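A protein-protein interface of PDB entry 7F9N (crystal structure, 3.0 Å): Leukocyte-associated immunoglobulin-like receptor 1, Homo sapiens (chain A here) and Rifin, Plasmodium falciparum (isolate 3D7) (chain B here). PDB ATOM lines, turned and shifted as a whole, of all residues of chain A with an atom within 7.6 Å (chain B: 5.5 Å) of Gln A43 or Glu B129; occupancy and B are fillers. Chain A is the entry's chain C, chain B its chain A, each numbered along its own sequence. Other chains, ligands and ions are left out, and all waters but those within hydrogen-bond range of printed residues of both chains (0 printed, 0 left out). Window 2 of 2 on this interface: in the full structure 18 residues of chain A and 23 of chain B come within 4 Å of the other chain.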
ATOM      1  N   PRO A  39     -10.060  -5.107  23.515  1.00  0.00           N
ATOM      2  CA  PRO A  39      -9.376  -6.218  24.171  1.00  0.00           C
ATOM      3  C   PRO A  39      -8.347  -5.818  25.201  1.00  0.00           C
ATOM      4  O   PRO A  39      -8.317  -4.706  25.726  1.00  0.00           O
ATOM      5  CB  PRO A  39      -8.711  -6.962  23.006  1.00  0.00           C
ATOM      6  CG  PRO A  39      -8.585  -6.007  21.954  1.00  0.00           C
ATOM      7  CD  PRO A  39      -9.763  -5.069  22.077  1.00  0.00           C
ATOM      8  N   VAL A  40      -7.540  -6.786  25.529  1.00  0.00           N
ATOM      9  CA  VAL A  40      -6.444  -6.613  26.463  1.00  0.00           C
ATOM     10  C   VAL A  40      -5.288  -5.943  25.722  1.00  0.00           C
ATOM     11  O   VAL A  40      -5.114  -6.116  24.506  1.00  0.00           O
ATOM     12  CB  VAL A  40      -6.075  -7.995  27.056  1.00  0.00           C
ATOM     13  CG1 VAL A  40      -5.924  -9.042  25.945  1.00  0.00           C
ATOM     14  CG2 VAL A  40      -4.848  -7.938  27.958  1.00  0.00           C
ATOM     15  N   GLY A  41      -4.522  -5.124  26.437  1.00  0.00           N
ATOM     16  CA  GLY A  41      -3.321  -4.560  25.858  1.00  0.00           C
ATOM     17  C   GLY A  41      -3.556  -3.390  24.926  1.00  0.00           C
ATOM     18  O   GLY A  41      -2.838  -3.230  23.925  1.00  0.00           O
ATOM     19  N   VAL A  42      -4.535  -2.563  25.221  1.00  0.00           N
ATOM     20  CA  VAL A  42      -4.784  -1.369  24.438  1.00  0.00           C
ATOM     21  C   VAL A  42      -3.973  -0.232  25.050  1.00  0.00           C
ATOM     22  O   VAL A  42      -3.967  -0.051  26.276  1.00  0.00           O
ATOM     23  CB  VAL A  42      -6.287  -1.054  24.409  1.00  0.00           C
ATOM     24  CG1 VAL A  42      -6.528   0.408  24.113  1.00  0.00           C
ATOM     25  CG2 VAL A  42      -6.964  -1.934  23.393  1.00  0.00           C
ATOM     26  N   GLN A  43      -3.248   0.509  24.208  1.00  0.00           N
ATOM     27  CA  GLN A  43      -2.439   1.601  24.734  1.00  0.00           C
ATOM     28  C   GLN A  43      -3.259   2.878  24.896  1.00  0.00           C
ATOM     29  O   GLN A  43      -3.288   3.486  25.983  1.00  0.00           O
ATOM     30  CB  GLN A  43      -1.240   1.846  23.821  1.00  0.00           C
ATOM     31  CG  GLN A  43      -0.416   3.069  24.250  1.00  0.00           C
ATOM     32  CD  GLN A  43       0.626   3.495  23.222  1.00  0.00           C
ATOM     33  OE1 GLN A  43       1.270   2.660  22.578  1.00  0.00           O
ATOM     34  NE2 GLN A  43       0.789   4.805  23.063  1.00  0.00           N
ATOM     35  N   THR A  44      -3.931   3.283  23.821  1.00  0.00           N
ATOM     36  CA  THR A  44      -4.697   4.514  23.781  1.00  0.00           C
ATOM     37  C   THR A  44      -6.092   4.182  23.296  1.00  0.00           C
ATOM     38  O   THR A  44      -6.263   3.382  22.361  1.00  0.00           O
ATOM     39  CB  THR A  44      -4.066   5.578  22.812  1.00  0.00           C
ATOM     40  OG1 THR A  44      -2.704   5.854  23.182  1.00  0.00           O
ATOM     41  CG2 THR A  44      -4.847   6.896  22.831  1.00  0.00           C
ATOM     42  N   PHE A  45      -7.085   4.796  23.936  1.00  0.00           N
ATOM     43  CA  PHE A  45      -8.445   4.825  23.420  1.00  0.00           C
ATOM     44  C   PHE A  45      -8.714   6.216  22.861  1.00  0.00           C
ATOM     45  O   PHE A  45      -8.217   7.223  23.388  1.00  0.00           O
ATOM     46  CB  PHE A  45      -9.475   4.466  24.505  1.00  0.00           C
ATOM     47  CG  PHE A  45      -9.775   2.984  24.583  1.00  0.00           C
ATOM     48  CD1 PHE A  45     -10.605   2.361  23.643  1.00  0.00           C
ATOM     49  CD2 PHE A  45      -9.216   2.213  25.596  1.00  0.00           C
ATOM     50  CE1 PHE A  45     -10.869   1.003  23.722  1.00  0.00           C
ATOM     51  CE2 PHE A  45      -9.473   0.861  25.677  1.00  0.00           C
ATOM     52  CZ  PHE A  45     -10.294   0.252  24.741  1.00  0.00           C
ATOM     53  N   ASP A  57      -8.181  11.412  23.414  1.00  0.00           N
ATOM     54  CA  ASP A  57      -7.285  10.275  23.588  1.00  0.00           C
ATOM     55  C   ASP A  57      -6.957  10.127  25.061  1.00  0.00           C
ATOM     56  O   ASP A  57      -6.579  11.113  25.713  1.00  0.00           O
ATOM     57  CB  ASP A  57      -5.978  10.457  22.821  1.00  0.00           C
ATOM     58  CG  ASP A  57      -6.063   9.948  21.417  1.00  0.00           C
ATOM     59  OD1 ASP A  57      -7.173   9.951  20.858  1.00  0.00           O
ATOM     60  OD2 ASP A  57      -5.035   9.520  20.875  1.00  0.00           O
ATOM     61  N   THR A  58      -7.096   8.907  25.591  1.00  0.00           N
ATOM     62  CA  THR A  58      -6.699   8.660  26.968  1.00  0.00           C
ATOM     63  C   THR A  58      -5.788   7.443  27.058  1.00  0.00           C
ATOM     64  O   THR A  58      -5.861   6.501  26.250  1.00  0.00           O
ATOM     65  CB  THR A  58      -7.903   8.502  27.916  1.00  0.00           C
ATOM     66  OG1 THR A  58      -7.492   8.827  29.249  1.00  0.00           O
ATOM     67  CG2 THR A  58      -8.425   7.095  27.912  1.00  0.00           C
ATOM     68  N   GLU A  59      -4.876   7.535  28.023  1.00  0.00           N
ATOM     69  CA  GLU A  59      -3.985   6.472  28.450  1.00  0.00           C
ATOM     70  C   GLU A  59      -4.448   5.864  29.760  1.00  0.00           C
ATOM     71  O   GLU A  59      -3.909   4.833  30.175  1.00  0.00           O
ATOM     72  CB  GLU A  59      -2.561   7.031  28.620  1.00  0.00           C
ATOM     73  CG  GLU A  59      -2.129   8.054  27.551  1.00  0.00           C
ATOM     74  CD  GLU A  59      -2.234   7.498  26.133  1.00  0.00           C
ATOM     75  OE1 GLU A  59      -2.464   8.284  25.187  1.00  0.00           O
ATOM     76  OE2 GLU A  59      -2.095   6.264  25.963  1.00  0.00           O
ATOM     77  N   ASP A  60      -5.428   6.502  30.414  1.00  0.00           N
ATOM     78  CA  ASP A  60      -6.058   6.029  31.653  1.00  0.00           C
ATOM     79  C   ASP A  60      -7.051   4.905  31.326  1.00  0.00           C
ATOM     80  O   ASP A  60      -8.276   5.039  31.444  1.00  0.00           O
ATOM     81  CB  ASP A  60      -6.731   7.202  32.360  1.00  0.00           C
ATOM     82  CG  ASP A  60      -6.848   7.006  33.860  1.00  0.00           C
ATOM     83  OD1 ASP A  60      -6.071   7.635  34.614  1.00  0.00           O
ATOM     84  OD2 ASP A  60      -7.727   6.229  34.286  1.00  0.00           O
ATOM     85  N   VAL A  61      -6.483   3.768  30.888  1.00  0.00           N
ATOM     86  CA  VAL A  61      -7.250   2.571  30.554  1.00  0.00           C
ATOM     87  C   VAL A  61      -7.392   1.697  31.796  1.00  0.00           C
ATOM     88  O   VAL A  61      -6.421   1.455  32.525  1.00  0.00           O
ATOM     89  CB  VAL A  61      -6.595   1.796  29.392  1.00  0.00           C
ATOM     90  CG1 VAL A  61      -5.103   1.638  29.615  1.00  0.00           C
ATOM     91  CG2 VAL A  61      -7.238   0.420  29.226  1.00  0.00           C
ATOM     92  N   SER A  69     -10.689  -4.553  28.178  1.00  0.00           N
ATOM     93  CA  SER A  69     -10.342  -3.344  28.907  1.00  0.00           C
ATOM     94  C   SER A  69     -11.182  -2.189  28.379  1.00  0.00           C
ATOM     95  O   SER A  69     -11.799  -2.265  27.311  1.00  0.00           O
ATOM     96  CB  SER A  69      -8.853  -3.023  28.804  1.00  0.00           C
ATOM     97  OG  SER A  69      -8.445  -2.995  27.448  1.00  0.00           O
ATOM     98  N   TYR A  90      -9.476   2.101  19.282  1.00  0.00           N
ATOM     99  CA  TYR A  90      -8.358   1.900  20.179  1.00  0.00           C
ATOM    100  C   TYR A  90      -7.090   1.673  19.373  1.00  0.00           C
ATOM    101  O   TYR A  90      -7.116   1.093  18.279  1.00  0.00           O
ATOM    102  CB  TYR A  90      -8.639   0.757  21.131  1.00  0.00           C
ATOM    103  CG  TYR A  90      -8.763  -0.597  20.481  1.00  0.00           C
ATOM    104  CD1 TYR A  90     -10.003  -1.149  20.195  1.00  0.00           C
ATOM    105  CD2 TYR A  90      -7.633  -1.342  20.190  1.00  0.00           C
ATOM    106  CE1 TYR A  90     -10.100  -2.407  19.619  1.00  0.00           C
ATOM    107  CE2 TYR A  90      -7.716  -2.585  19.628  1.00  0.00           C
ATOM    108  CZ  TYR A  90      -8.940  -3.115  19.337  1.00  0.00           C
ATOM    109  OH  TYR A  90      -8.990  -4.362  18.760  1.00  0.00           O
ATOM    110  N   TYR A  91      -5.980   2.146  19.909  1.00  0.00           N
ATOM    111  CA  TYR A  91      -4.699   1.966  19.250  1.00  0.00           C
ATOM    112  C   TYR A  91      -3.968   0.895  20.028  1.00  0.00           C
ATOM    113  O   TYR A  91      -3.602   1.100  21.194  1.00  0.00           O
ATOM    114  CB  TYR A  91      -3.894   3.269  19.171  1.00  0.00           C
ATOM    115  CG  TYR A  91      -2.547   3.164  18.454  1.00  0.00           C
ATOM    116  CD1 TYR A  91      -2.472   3.057  17.067  1.00  0.00           C
ATOM    117  CD2 TYR A  91      -1.349   3.198  19.167  1.00  0.00           C
ATOM    118  CE1 TYR A  91      -1.231   2.976  16.405  1.00  0.00           C
ATOM    119  CE2 TYR A  91      -0.106   3.126  18.516  1.00  0.00           C
ATOM    120  CZ  TYR A  91      -0.051   3.013  17.134  1.00  0.00           C
ATOM    121  OH  TYR A  91       1.171   2.925  16.485  1.00  0.00           O
ATOM    122  N   LYS A  92      -3.798  -0.251  19.395  1.00  0.00           N
ATOM    123  CA  LYS A  92      -2.947  -1.277  19.966  1.00  0.00           C
ATOM    124  C   LYS A  92      -1.731  -1.374  19.077  1.00  0.00           C
ATOM    125  O   LYS A  92      -1.850  -1.842  17.931  1.00  0.00           O
ATOM    126  CB  LYS A  92      -3.646  -2.634  20.066  1.00  0.00           C
ATOM    127  CG  LYS A  92      -2.670  -3.754  20.383  1.00  0.00           C
ATOM    128  CD  LYS A  92      -3.208  -4.733  21.387  1.00  0.00           C
ATOM    129  CE  LYS A  92      -4.247  -5.620  20.758  1.00  0.00           C
ATOM    130  NZ  LYS A  92      -4.633  -6.776  21.645  1.00  0.00           N
ATOM    131  N   PRO A  93      -0.571  -0.926  19.557  1.00  0.00           N
ATOM    132  CA  PRO A  93       0.631  -0.819  18.703  1.00  0.00           C
ATOM    133  C   PRO A  93       0.832  -2.074  17.874  1.00  0.00           C
ATOM    134  O   PRO A  93       0.603  -3.198  18.356  1.00  0.00           O
ATOM    135  CB  PRO A  93       1.764  -0.631  19.722  1.00  0.00           C
ATOM    136  CG  PRO A  93       1.092   0.078  20.876  1.00  0.00           C
ATOM    137  CD  PRO A  93      -0.327  -0.445  20.933  1.00  0.00           C
ATOM    138  N   PRO A  94       1.210  -1.918  16.601  1.00  0.00           N
ATOM    139  CA  PRO A  94       1.481  -0.609  16.008  1.00  0.00           C
ATOM    140  C   PRO A  94       0.317  -0.005  15.217  1.00  0.00           C
ATOM    141  O   PRO A  94       0.533   1.008  14.531  1.00  0.00           O
ATOM    142  CB  PRO A  94       2.634  -0.908  15.052  1.00  0.00           C
ATOM    143  CG  PRO A  94       2.581  -2.432  14.828  1.00  0.00           C
ATOM    144  CD  PRO A  94       1.442  -2.989  15.625  1.00  0.00           C
ATOM    145  N   LEU B 125      -1.688   8.543  14.423  1.00  0.00           N
ATOM    146  CA  LEU B 125      -1.159   7.831  15.569  1.00  0.00           C
ATOM    147  C   LEU B 125      -1.479   8.592  16.844  1.00  0.00           C
ATOM    148  O   LEU B 125      -1.689   9.810  16.809  1.00  0.00           O
ATOM    149  CB  LEU B 125       0.346   7.581  15.449  1.00  0.00           C
ATOM    150  CG  LEU B 125       1.299   8.680  15.151  1.00  0.00           C
ATOM    151  CD1 LEU B 125       2.569   8.155  15.727  1.00  0.00           C
ATOM    152  CD2 LEU B 125       1.383   8.870  13.625  1.00  0.00           C
ATOM    153  N   PRO B 126      -1.550   7.875  17.992  1.00  0.00           N
ATOM    154  CA  PRO B 126      -2.425   8.317  19.076  1.00  0.00           C
ATOM    155  C   PRO B 126      -2.030   9.553  19.842  1.00  0.00           C
ATOM    156  O   PRO B 126      -2.077   9.479  21.082  1.00  0.00           O
ATOM    157  CB  PRO B 126      -2.406   7.126  20.031  1.00  0.00           C
ATOM    158  CG  PRO B 126      -1.115   6.472  19.785  1.00  0.00           C
ATOM    159  CD  PRO B 126      -0.969   6.561  18.312  1.00  0.00           C
ATOM    160  N   ASP B 127      -1.632  10.659  19.202  1.00  0.00           N
ATOM    161  CA  ASP B 127      -1.693  11.921  19.931  1.00  0.00           C
ATOM    162  C   ASP B 127      -0.600  11.995  20.987  1.00  0.00           C
ATOM    163  O   ASP B 127      -0.250  13.075  21.462  1.00  0.00           O
ATOM    164  CB  ASP B 127      -3.085  12.065  20.572  1.00  0.00           C
ATOM    165  CG  ASP B 127      -3.494  13.487  20.788  1.00  0.00           C
ATOM    166  OD1 ASP B 127      -2.806  14.191  21.560  1.00  0.00           O
ATOM    167  OD2 ASP B 127      -4.520  13.901  20.205  1.00  0.00           O
ATOM    168  N   LYS B 128      -0.085  10.843  21.389  1.00  0.00           N
ATOM    169  CA  LYS B 128       0.980  10.731  22.368  1.00  0.00           C
ATOM    170  C   LYS B 128       2.287  10.384  21.713  1.00  0.00           C
ATOM    171  O   LYS B 128       3.341  10.763  22.215  1.00  0.00           O
ATOM    172  CB  LYS B 128       0.642   9.651  23.407  1.00  0.00           C
ATOM    173  CG  LYS B 128       1.709   9.385  24.461  1.00  0.00           C
ATOM    174  CD  LYS B 128       1.277   8.252  25.399  1.00  0.00           C
ATOM    175  CE  LYS B 128       2.249   8.089  26.564  1.00  0.00           C
ATOM    176  NZ  LYS B 128       1.672   7.241  27.663  1.00  0.00           N
ATOM    177  N   GLU B 129       2.220   9.662  20.605  1.00  0.00           N
ATOM    178  CA  GLU B 129       3.378   9.383  19.780  1.00  0.00           C
ATOM    179  C   GLU B 129       3.604  10.481  18.742  1.00  0.00           C
ATOM    180  O   GLU B 129       4.753  10.815  18.429  1.00  0.00           O
ATOM    181  CB  GLU B 129       3.181   8.026  19.098  1.00  0.00           C
ATOM    182  CG  GLU B 129       3.579   6.808  19.907  1.00  0.00           C
ATOM    183  CD  GLU B 129       2.559   6.384  20.969  1.00  0.00           C
ATOM    184  OE1 GLU B 129       1.774   7.230  21.475  1.00  0.00           O
ATOM    185  OE2 GLU B 129       2.539   5.169  21.287  1.00  0.00           O
ATOM    186  N   ALA B 130       2.513  11.074  18.251  1.00  0.00           N
ATOM    187  CA  ALA B 130       2.581  12.026  17.159  1.00  0.00           C
ATOM    188  C   ALA B 130       3.232  13.313  17.605  1.00  0.00           C
ATOM    189  O   ALA B 130       4.191  13.791  16.976  1.00  0.00           O
ATOM    190  CB  ALA B 130       1.182  12.307  16.628  1.00  0.00           C
ATOM    191  N   VAL B 131       2.714  13.907  18.674  1.00  0.00           N
ATOM    192  CA  VAL B 131       3.230  15.209  19.091  1.00  0.00           C
ATOM    193  C   VAL B 131       4.740  15.215  19.235  1.00  0.00           C
ATOM    194  O   VAL B 131       5.398  15.960  18.489  1.00  0.00           O
ATOM    195  CB  VAL B 131       2.495  15.685  20.366  1.00  0.00           C
ATOM    196  CG1 VAL B 131       3.117  16.933  20.922  1.00  0.00           C
ATOM    197  CG2 VAL B 131       1.092  15.970  19.983  1.00  0.00           C
ATOM    198  N   PRO B 132       5.371  14.380  20.061  1.00  0.00           N
ATOM    199  CA  PRO B 132       6.838  14.361  20.054  1.00  0.00           C
ATOM    200  C   PRO B 132       7.421  14.048  18.686  1.00  0.00           C
ATOM    201  O   PRO B 132       8.482  14.582  18.344  1.00  0.00           O
ATOM    202  CB  PRO B 132       7.188  13.270  21.076  1.00  0.00           C
ATOM    203  CG  PRO B 132       5.950  13.111  21.892  1.00  0.00           C
ATOM    204  CD  PRO B 132       4.846  13.298  20.910  1.00  0.00           C
ATOM    205  N   LYS B 133       6.746  13.218  17.884  1.00  0.00           N
ATOM    206  CA  LYS B 133       7.300  12.865  16.582  1.00  0.00           C
ATOM    207  C   LYS B 133       7.416  14.085  15.675  1.00  0.00           C
ATOM    208  O   LYS B 133       8.446  14.274  15.019  1.00  0.00           O
ATOM    209  CB  LYS B 133       6.461  11.776  15.918  1.00  0.00           C
ATOM    210  CG  LYS B 133       7.028  11.278  14.598  1.00  0.00           C
ATOM    211  CD  LYS B 133       6.444   9.920  14.228  1.00  0.00           C
ATOM    212  CE  LYS B 133       6.954   9.383  12.889  1.00  0.00           C
ATOM    213  NZ  LYS B 133       6.641  10.278  11.728  1.00  0.00           N
ATOM    214  N   VAL B 134       6.386  14.932  15.624  1.00  0.00           N
ATOM    215  CA  VAL B 134       6.498  16.089  14.742  1.00  0.00           C
ATOM    216  C   VAL B 134       7.476  17.097  15.320  1.00  0.00           C
ATOM    217  O   VAL B 134       8.224  17.726  14.569  1.00  0.00           O
ATOM    218  CB  VAL B 134       5.134  16.744  14.447  1.00  0.00           C
ATOM    219  CG1 VAL B 134       4.713  17.674  15.550  1.00  0.00           C
ATOM    220  CG2 VAL B 134       5.193  17.508  13.157  1.00  0.00           C
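The side-chain amide nitrogen of Gln A43 lies within hydrogen-bond range of the side-chain carboxylate of Glu B129 (2.5 Å). The side-chain carboxylate of Asp A57 lies close to the backbone carbonyl oxygen of Pro B126, 3.0 Å away.
O of Tyr A91 sits at hydrogen-bond distance from N of Gln A43 (3.1 Å). OE2 of Glu A59 sits at hydrogen-bond distance from OG1 of Thr A44, at 2.9 Å. The backbone carbonyl oxygen (O) of Thr A44 sits at hydrogen-bond distance from the backbone NH (N) of Tyr A91 (2.8 Å). The side-chain hydroxyl (OH) of Tyr A91 lies within hydrogen-bond range of the backbone carbonyl oxygen (O) of Pro A94 (2.8 Å).
Among the printed residues, merely in contact across the chains: Asp A57 with Asp B127 (3.2 Å), Tyr A91 with Pro B126 (3.3 Å), Thr A44 with Pro B126 (3.4 Å) and Glu A59 with Lys B128 (3.7 Å).
Gln A43 touches one residue of chain B. Tyr A90 touches none of the printed residues of chain B. Printed residues of chain B within 4 Å of Tyr A91: Pro B126. Of the printed residues of chain A, Pro B126 touches Thr A44, Asp A57 and Tyr A91. Glu B129 touches just one residue of chain A: Gln A43. Val B131 touches none of the printed residues of chain A.
Of the 10 printed residues of chain B, 4 touch a printed residue of chain A. Of the 18 printed residues of chain A, 5 touch a printed residue of chain B. Among the printed residues, no Asp or Glu carboxylate lies within 4 Å of a Lys or Arg side-chain nitrogen of the other chain.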
